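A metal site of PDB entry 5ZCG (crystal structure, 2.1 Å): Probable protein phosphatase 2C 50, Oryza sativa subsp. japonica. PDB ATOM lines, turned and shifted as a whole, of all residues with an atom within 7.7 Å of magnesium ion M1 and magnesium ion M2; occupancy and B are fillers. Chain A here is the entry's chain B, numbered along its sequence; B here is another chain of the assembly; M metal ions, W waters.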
ATOM      1  N   SER A  13       4.089   5.405  14.418  1.00  0.00           N
ATOM      2  CA  SER A  13       2.793   5.377  15.091  1.00  0.00           C
ATOM      3  C   SER A  13       1.675   5.646  14.096  1.00  0.00           C
ATOM      4  O   SER A  13       1.866   6.301  13.067  1.00  0.00           O
ATOM      5  CB  SER A  13       2.755   6.392  16.226  1.00  0.00           C
ATOM      6  OG  SER A  13       3.525   5.960  17.340  1.00  0.00           O
ATOM      7  N   GLU A  15      -1.312   7.371  14.392  1.00  0.00           N
ATOM      8  CA  GLU A  15      -1.768   8.749  14.589  1.00  0.00           C
ATOM      9  C   GLU A  15      -0.662   9.676  15.086  1.00  0.00           C
ATOM     10  O   GLU A  15       0.254   9.286  15.837  1.00  0.00           O
ATOM     11  CB  GLU A  15      -2.944   8.786  15.593  1.00  0.00           C
ATOM     12  CG  GLU A  15      -4.123   7.903  15.205  1.00  0.00           C
ATOM     13  CD  GLU A  15      -5.484   8.596  15.476  1.00  0.00           C
ATOM     14  OE1 GLU A  15      -5.865   9.748  15.053  1.00  0.00           O
ATOM     15  OE2 GLU A  15      -6.306   7.724  15.873  1.00  0.00           O
ATOM     16  N   MET A  16      -0.789  10.941  14.691  1.00  0.00           N
ATOM     17  CA  MET A  16       0.085  12.018  15.137  1.00  0.00           C
ATOM     18  C   MET A  16      -0.553  12.717  16.330  1.00  0.00           C
ATOM     19  O   MET A  16      -1.672  13.245  16.212  1.00  0.00           O
ATOM     20  CB  MET A  16       0.345  13.016  13.991  1.00  0.00           C
ATOM     21  CG  MET A  16       1.254  14.179  14.402  1.00  0.00           C
ATOM     22  SD  MET A  16       2.791  13.603  15.184  1.00  0.00           S
ATOM     23  CE  MET A  16       3.948  14.874  14.655  1.00  0.00           C
ATOM     24  N   GLU A  17       0.146  12.734  17.452  1.00  0.00           N
ATOM     25  CA  GLU A  17      -0.360  13.415  18.630  1.00  0.00           C
ATOM     26  C   GLU A  17       0.630  14.404  19.223  1.00  0.00           C
ATOM     27  O   GLU A  17       0.335  15.027  20.249  1.00  0.00           O
ATOM     28  CB  GLU A  17      -0.790  12.384  19.692  1.00  0.00           C
ATOM     29  CG  GLU A  17      -1.987  11.544  19.217  1.00  0.00           C
ATOM     30  CD  GLU A  17      -2.403  10.492  20.217  1.00  0.00           C
ATOM     31  OE1 GLU A  17      -3.562  10.015  20.140  1.00  0.00           O
ATOM     32  OE2 GLU A  17      -1.568  10.131  21.076  1.00  0.00           O
ATOM     33  N   ASP A  18       1.792  14.569  18.597  1.00  0.00           N
ATOM     34  CA  ASP A  18       2.690  15.653  18.932  1.00  0.00           C
ATOM     35  C   ASP A  18       2.190  16.940  18.309  1.00  0.00           C
ATOM     36  O   ASP A  18       1.596  16.939  17.223  1.00  0.00           O
ATOM     37  CB  ASP A  18       4.103  15.358  18.407  1.00  0.00           C
ATOM     38  CG  ASP A  18       4.910  14.436  19.315  1.00  0.00           C
ATOM     39  OD1 ASP A  18       4.361  13.893  20.302  1.00  0.00           O
ATOM     40  OD2 ASP A  18       6.117  14.262  19.034  1.00  0.00           O
ATOM     41  N   ALA A  19       2.414  18.046  19.009  1.00  0.00           N
ATOM     42  CA  ALA A  19       2.188  19.384  18.492  1.00  0.00           C
ATOM     43  C   ALA A  19       3.399  20.231  18.858  1.00  0.00           C
ATOM     44  O   ALA A  19       4.195  19.871  19.731  1.00  0.00           O
ATOM     45  CB  ALA A  19       0.909  20.013  19.061  1.00  0.00           C
ATOM     46  N   PHE A  60       4.742  19.850  22.603  1.00  0.00           N
ATOM     47  CA  PHE A  60       3.645  19.310  23.394  1.00  0.00           C
ATOM     48  C   PHE A  60       3.362  17.900  22.921  1.00  0.00           C
ATOM     49  O   PHE A  60       2.845  17.689  21.813  1.00  0.00           O
ATOM     50  CB  PHE A  60       2.422  20.213  23.267  1.00  0.00           C
ATOM     51  CG  PHE A  60       2.764  21.698  23.299  1.00  0.00           C
ATOM     52  CD1 PHE A  60       2.970  22.348  24.508  1.00  0.00           C
ATOM     53  CD2 PHE A  60       2.905  22.419  22.126  1.00  0.00           C
ATOM     54  CE1 PHE A  60       3.300  23.702  24.545  1.00  0.00           C
ATOM     55  CE2 PHE A  60       3.234  23.773  22.163  1.00  0.00           C
ATOM     56  CZ  PHE A  60       3.433  24.408  23.372  1.00  0.00           C
ATOM     57  N   ASP A  61       3.696  16.917  23.740  1.00  0.00           N
ATOM     58  CA  ASP A  61       3.553  15.511  23.389  1.00  0.00           C
ATOM     59  C   ASP A  61       2.226  15.029  23.984  1.00  0.00           C
ATOM     60  O   ASP A  61       2.136  14.777  25.183  1.00  0.00           O
ATOM     61  CB  ASP A  61       4.737  14.725  23.928  1.00  0.00           C
ATOM     62  CG  ASP A  61       4.684  13.251  23.579  1.00  0.00           C
ATOM     63  OD1 ASP A  61       3.676  12.775  22.990  1.00  0.00           O
ATOM     64  OD2 ASP A  61       5.663  12.562  23.913  1.00  0.00           O
ATOM     65  N   GLY A  62       1.214  14.902  23.132  1.00  0.00           N
ATOM     66  CA  GLY A  62      -0.087  14.472  23.606  1.00  0.00           C
ATOM     67  C   GLY A  62      -0.189  12.964  23.728  1.00  0.00           C
ATOM     68  O   GLY A  62       0.422  12.199  22.993  1.00  0.00           O
ATOM     69  N   HIS A  63      -1.001  12.534  24.693  1.00  0.00           N
ATOM     70  CA  HIS A  63      -1.356  11.133  24.864  1.00  0.00           C
ATOM     71  C   HIS A  63      -2.862  11.042  25.076  1.00  0.00           C
ATOM     72  O   HIS A  63      -3.496  11.996  25.551  1.00  0.00           O
ATOM     73  CB  HIS A  63      -0.618  10.489  26.052  1.00  0.00           C
ATOM     74  CG  HIS A  63      -0.708  11.283  27.319  1.00  0.00           C
ATOM     75  ND1 HIS A  63       0.237  12.212  27.691  1.00  0.00           N
ATOM     76  CD2 HIS A  63      -1.648  11.287  28.306  1.00  0.00           C
ATOM     77  CE1 HIS A  63      -0.100  12.758  28.846  1.00  0.00           C
ATOM     78  NE2 HIS A  63      -1.243  12.212  29.242  1.00  0.00           N
ATOM     79  N   GLY A  64      -3.431   9.901  24.714  1.00  0.00           N
ATOM     80  CA  GLY A  64      -4.866   9.733  24.714  1.00  0.00           C
ATOM     81  C   GLY A  64      -5.583  10.464  23.610  1.00  0.00           C
ATOM     82  O   GLY A  64      -6.818  10.380  23.521  1.00  0.00           O
ATOM     83  N   GLY A  65      -4.864  11.178  22.763  1.00  0.00           N
ATOM     84  CA  GLY A  65      -5.434  12.046  21.748  1.00  0.00           C
ATOM     85  C   GLY A  65      -4.510  13.217  21.491  1.00  0.00           C
ATOM     86  O   GLY A  65      -3.511  13.417  22.179  1.00  0.00           O
ATOM     87  N   ALA A  66      -4.875  14.009  20.481  1.00  0.00           N
ATOM     88  CA  ALA A  66      -4.103  15.176  20.088  1.00  0.00           C
ATOM     89  C   ALA A  66      -4.655  16.492  20.625  1.00  0.00           C
ATOM     90  O   ALA A  66      -4.006  17.534  20.457  1.00  0.00           O
ATOM     91  CB  ALA A  66      -3.994  15.243  18.562  1.00  0.00           C
ATOM     92  N   ALA A  69      -2.620  18.572  23.362  1.00  0.00           N
ATOM     93  CA  ALA A  69      -1.393  19.081  22.734  1.00  0.00           C
ATOM     94  C   ALA A  69      -1.697  20.239  21.797  1.00  0.00           C
ATOM     95  O   ALA A  69      -0.979  21.250  21.795  1.00  0.00           O
ATOM     96  CB  ALA A  69      -0.681  17.949  22.002  1.00  0.00           C
ATOM     97  N   GLY A 143      -4.184  14.070  27.711  1.00  0.00           N
ATOM     98  CA  GLY A 143      -3.214  14.971  28.300  1.00  0.00           C
ATOM     99  C   GLY A 143      -2.117  15.316  27.319  1.00  0.00           C
ATOM    100  O   GLY A 143      -2.163  14.940  26.137  1.00  0.00           O
ATOM    101  N   SER A 144      -1.129  16.058  27.804  1.00  0.00           N
ATOM    102  CA  SER A 144       0.009  16.412  26.983  1.00  0.00           C
ATOM    103  C   SER A 144       1.155  16.873  27.879  1.00  0.00           C
ATOM    104  O   SER A 144       0.929  17.426  28.960  1.00  0.00           O
ATOM    105  CB  SER A 144      -0.336  17.494  25.967  1.00  0.00           C
ATOM    106  OG  SER A 144       0.822  17.969  25.318  1.00  0.00           O
ATOM    107  N   THR A 145       2.374  16.641  27.411  1.00  0.00           N
ATOM    108  CA  THR A 145       3.515  17.328  27.990  1.00  0.00           C
ATOM    109  C   THR A 145       3.551  18.768  27.484  1.00  0.00           C
ATOM    110  O   THR A 145       2.817  19.154  26.576  1.00  0.00           O
ATOM    111  CB  THR A 145       4.825  16.622  27.640  1.00  0.00           C
ATOM    112  OG1 THR A 145       5.172  16.908  26.275  1.00  0.00           O
ATOM    113  CG2 THR A 145       4.726  15.106  27.847  1.00  0.00           C
ATOM    114  N   ASP A 163       7.694  14.621  30.239  1.00  0.00           N
ATOM    115  CA  ASP A 163       8.904  13.923  29.833  1.00  0.00           C
ATOM    116  C   ASP A 163       9.412  14.359  28.456  1.00  0.00           C
ATOM    117  O   ASP A 163      10.228  13.655  27.859  1.00  0.00           O
ATOM    118  CB  ASP A 163       8.698  12.405  29.863  1.00  0.00           C
ATOM    119  CG  ASP A 163       7.556  11.929  28.980  1.00  0.00           C
ATOM    120  OD1 ASP A 163       7.149  12.639  28.027  1.00  0.00           O
ATOM    121  OD2 ASP A 163       7.053  10.816  29.242  1.00  0.00           O
ATOM    122  N   SER A 164       8.918  15.472  27.925  1.00  0.00           N
ATOM    123  CA  SER A 164       9.644  16.124  26.856  1.00  0.00           C
ATOM    124  C   SER A 164      10.870  16.812  27.458  1.00  0.00           C
ATOM    125  O   SER A 164      11.009  16.929  28.682  1.00  0.00           O
ATOM    126  CB  SER A 164       8.759  17.119  26.110  1.00  0.00           C
ATOM    127  OG  SER A 164       7.642  16.466  25.516  1.00  0.00           O
ATOM    128  N   MET A 213       4.535   9.435  33.255  1.00  0.00           N
ATOM    129  CA  MET A 213       5.032  10.745  33.635  1.00  0.00           C
ATOM    130  C   MET A 213       4.228  11.244  34.830  1.00  0.00           C
ATOM    131  O   MET A 213       3.030  10.963  34.956  1.00  0.00           O
ATOM    132  CB  MET A 213       4.994  11.750  32.479  1.00  0.00           C
ATOM    133  CG  MET A 213       3.636  12.359  32.196  1.00  0.00           C
ATOM    134  SD  MET A 213       3.616  13.082  30.545  1.00  0.00           S
ATOM    135  CE  MET A 213       3.949  11.630  29.557  1.00  0.00           C
ATOM    136  N   SER A 248      10.183  16.030  21.852  1.00  0.00           N
ATOM    137  CA  SER A 248       9.414  15.016  22.559  1.00  0.00           C
ATOM    138  C   SER A 248      10.292  13.792  22.820  1.00  0.00           C
ATOM    139  O   SER A 248      11.407  13.648  22.282  1.00  0.00           O
ATOM    140  CB  SER A 248       8.171  14.626  21.763  1.00  0.00           C
ATOM    141  OG  SER A 248       8.503  14.123  20.469  1.00  0.00           O
ATOM    142  N   ASP A 249       9.782  12.889  23.661  1.00  0.00           N
ATOM    143  CA  ASP A 249      10.566  11.708  24.019  1.00  0.00           C
ATOM    144  C   ASP A 249      10.818  10.789  22.838  1.00  0.00           C
ATOM    145  O   ASP A 249      11.686   9.917  22.937  1.00  0.00           O
ATOM    146  CB  ASP A 249       9.876  10.932  25.151  1.00  0.00           C
ATOM    147  CG  ASP A 249       8.459  10.495  24.802  1.00  0.00           C
ATOM    148  OD1 ASP A 249       7.972  10.810  23.698  1.00  0.00           O
ATOM    149  OD2 ASP A 249       7.835   9.842  25.661  1.00  0.00           O
ATOM    150  N   GLY A 250      10.121  10.980  21.713  1.00  0.00           N
ATOM    151  CA  GLY A 250      10.446  10.238  20.499  1.00  0.00           C
ATOM    152  C   GLY A 250      11.890  10.416  20.075  1.00  0.00           C
ATOM    153  O   GLY A 250      12.475   9.514  19.454  1.00  0.00           O
ATOM    154  N   LEU A 251      12.482  11.564  20.392  1.00  0.00           N
ATOM    155  CA  LEU A 251      13.902  11.767  20.181  1.00  0.00           C
ATOM    156  C   LEU A 251      14.712  11.254  21.362  1.00  0.00           C
ATOM    157  O   LEU A 251      15.608  10.415  21.186  1.00  0.00           O
ATOM    158  CB  LEU A 251      14.194  13.253  19.941  1.00  0.00           C
ATOM    159  CG  LEU A 251      15.673  13.588  19.698  1.00  0.00           C
ATOM    160  CD1 LEU A 251      16.179  12.888  18.431  1.00  0.00           C
ATOM    161  CD2 LEU A 251      15.911  15.102  19.605  1.00  0.00           C
ATOM    162  N   ASP A 253      14.229   9.227  23.732  1.00  0.00           N
ATOM    163  CA  ASP A 253      14.211   7.811  24.101  1.00  0.00           C
ATOM    164  C   ASP A 253      15.413   7.065  23.527  1.00  0.00           C
ATOM    165  O   ASP A 253      15.917   6.123  24.150  1.00  0.00           O
ATOM    166  CB  ASP A 253      12.919   7.145  23.626  1.00  0.00           C
ATOM    167  CG  ASP A 253      11.745   7.396  24.570  1.00  0.00           C
ATOM    168  OD1 ASP A 253      11.975   7.871  25.703  1.00  0.00           O
ATOM    169  OD2 ASP A 253      10.593   7.133  24.173  1.00  0.00           O
ATOM    170  N   SER A 309      13.143   4.394  17.156  1.00  0.00           N
ATOM    171  CA  SER A 309      12.061   5.036  17.904  1.00  0.00           C
ATOM    172  C   SER A 309      10.710   4.676  17.307  1.00  0.00           C
ATOM    173  O   SER A 309      10.487   4.818  16.104  1.00  0.00           O
ATOM    174  CB  SER A 309      12.252   6.555  17.912  1.00  0.00           C
ATOM    175  OG  SER A 309      11.124   7.202  18.487  1.00  0.00           O
ATOM    176  N   ASP A 311       7.825   6.107  18.467  1.00  0.00           N
ATOM    177  CA  ASP A 311       6.864   7.138  18.863  1.00  0.00           C
ATOM    178  C   ASP A 311       6.767   8.265  17.841  1.00  0.00           C
ATOM    179  O   ASP A 311       7.514   8.337  16.862  1.00  0.00           O
ATOM    180  CB  ASP A 311       7.302   7.730  20.203  1.00  0.00           C
ATOM    181  CG  ASP A 311       6.181   8.425  20.947  1.00  0.00           C
ATOM    182  OD1 ASP A 311       5.127   8.718  20.346  1.00  0.00           O
ATOM    183  OD2 ASP A 311       6.392   8.727  22.133  1.00  0.00           O
ATOM    184  N   ASN A 312       5.799   9.168  18.069  1.00  0.00           N
ATOM    185  CA  ASN A 312       5.813  10.458  17.402  1.00  0.00           C
ATOM    186  C   ASN A 312       7.127  11.172  17.720  1.00  0.00           C
ATOM    187  O   ASN A 312       7.679  11.038  18.815  1.00  0.00           O
ATOM    188  CB  ASN A 312       4.636  11.328  17.847  1.00  0.00           C
ATOM    189  CG  ASN A 312       3.286  10.744  17.475  1.00  0.00           C
ATOM    190  OD1 ASN A 312       2.256  11.157  18.008  1.00  0.00           O
ATOM    191  ND2 ASN A 312       3.287   9.780  16.558  1.00  0.00           N
ATOM    192  N   ILE A 313       7.640  11.923  16.757  1.00  0.00           N
ATOM    193  CA  ILE A 313       8.891  12.638  16.919  1.00  0.00           C
ATOM    194  C   ILE A 313       8.686  14.101  16.532  1.00  0.00           C
ATOM    195  O   ILE A 313       8.183  14.392  15.435  1.00  0.00           O
ATOM    196  CB  ILE A 313      10.026  12.014  16.064  1.00  0.00           C
ATOM    197  CG1 ILE A 313      10.198  10.524  16.412  1.00  0.00           C
ATOM    198  CG2 ILE A 313      11.325  12.750  16.300  1.00  0.00           C
ATOM    199  CD1 ILE A 313      10.873   9.720  15.304  1.00  0.00           C
ATOM    200  N   THR A 314       9.047  15.010  17.430  1.00  0.00           N
ATOM    201  CA  THR A 314       8.994  16.438  17.145  1.00  0.00           C
ATOM    202  C   THR A 314      10.280  17.054  17.674  1.00  0.00           C
ATOM    203  O   THR A 314      10.651  16.814  18.824  1.00  0.00           O
ATOM    204  CB  THR A 314       7.760  17.095  17.767  1.00  0.00           C
ATOM    205  OG1 THR A 314       6.580  16.612  17.111  1.00  0.00           O
ATOM    206  CG2 THR A 314       7.814  18.616  17.610  1.00  0.00           C
ATOM    207  N   SER B  71      -2.943   6.029  23.140  1.00  0.00           N
ATOM    208  CA  SER B  71      -1.553   6.174  23.512  1.00  0.00           C
ATOM    209  C   SER B  71      -1.411   6.595  24.977  1.00  0.00           C
ATOM    210  O   SER B  71      -2.371   7.003  25.642  1.00  0.00           O
ATOM    211  CB  SER B  71      -0.865   7.211  22.618  1.00  0.00           C
ATOM    212  OG  SER B  71      -1.545   8.466  22.703  1.00  0.00           O
HETATM  213 MG    MG M   1       6.043  10.712  22.876  1.00  0.00          MG
HETATM  214 MG    MG M   2       2.453  12.177  20.924  1.00  0.00          MG
HETATM  215  O   HOH W   1       1.054   9.884  21.632  1.00  0.00           O
HETATM  216  O   HOH W   2       6.309  11.819  21.170  1.00  0.00           O
HETATM  217  O   HOH W   3       5.494   9.624  24.339  1.00  0.00           O
HETATM  218  O   HOH W   4       4.226  10.134  22.382  1.00  0.00           O
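Within 4 Å of magnesium ion M1: Asp 61, Asp 249 and Asp 311.
The nearest printed residue that does not touch magnesium ion M1 is Gly 250 (4.2 Å).
C of Glu 17 touches magnesium ion M2 (3.3 Å).
Gly 62 touches magnesium ion M2.
OD1 of Asn 312 touches magnesium ion M2, 3.1 Å away.
Along chain A the residues within 4 Å of magnesium ion M2 span positions 17 to 312.
The nearest printed residue that does not touch magnesium ion M2 is Asp 311 (4.4 Å).
Magnesium ion M2 is bound by OD1 of Asp 61.
Magnesium ion M2 has one donor atom within binding distance.
Slightly farther from magnesium ion M2 lies the side-chain carboxylate (OD1) of Asp 18 (2.6 Å).
Slightly farther from magnesium ion M2 lies water W1 (2.8 Å).
Water W1 lies within hydrogen-bond range of OE2 of Glu 17 (2.7 Å), O of Gly 62 (2.8 Å) and OG of Ser 71 of chain B (3.1 Å).
N of Gly 62 sits at hydrogen-bond distance from O of Glu 17 (3.0 Å).
The backbone carbonyl oxygen of Glu 15 sits at hydrogen-bond distance from the side-chain amide nitrogen of Asn 312.
The side-chain amide oxygen (OD1) of Asn 312 sits close to the side-chain sulfur (SD) of Met 16 (3.8 Å).
The side-chain carboxylate (OE1) of Glu 17 is in hydrogen-bond range of the backbone NH (N) of Gly 65, 3.2 Å away.
N of Asp 18 is in hydrogen-bond range of OD1 of Asn 312, at 3.5 Å.
The backbone NH (N) of Thr 145 is in hydrogen-bond range of the backbone carbonyl oxygen (O) of Asp 61 (2.9 Å).
The side-chain hydroxyl (OG) of Ser 144 lies within hydrogen-bond range of the backbone NH (N) of Asp 61 (3.4 Å).
The side-chain carboxylate (OD2) of Asp 18 is in hydrogen-bond range of the side-chain hydroxyl (OG) of Ser 248, at 2.8 Å.
Magnesium ion M1 is bound by water W3 (1.9 Å), water W4 (2.0 Å), water W2 (2.1 Å), OD1 of Asp 249 (2.1 Å), OD2 of Asp 311 (2.1 Å) and OD2 of Asp 61 (2.2 Å).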
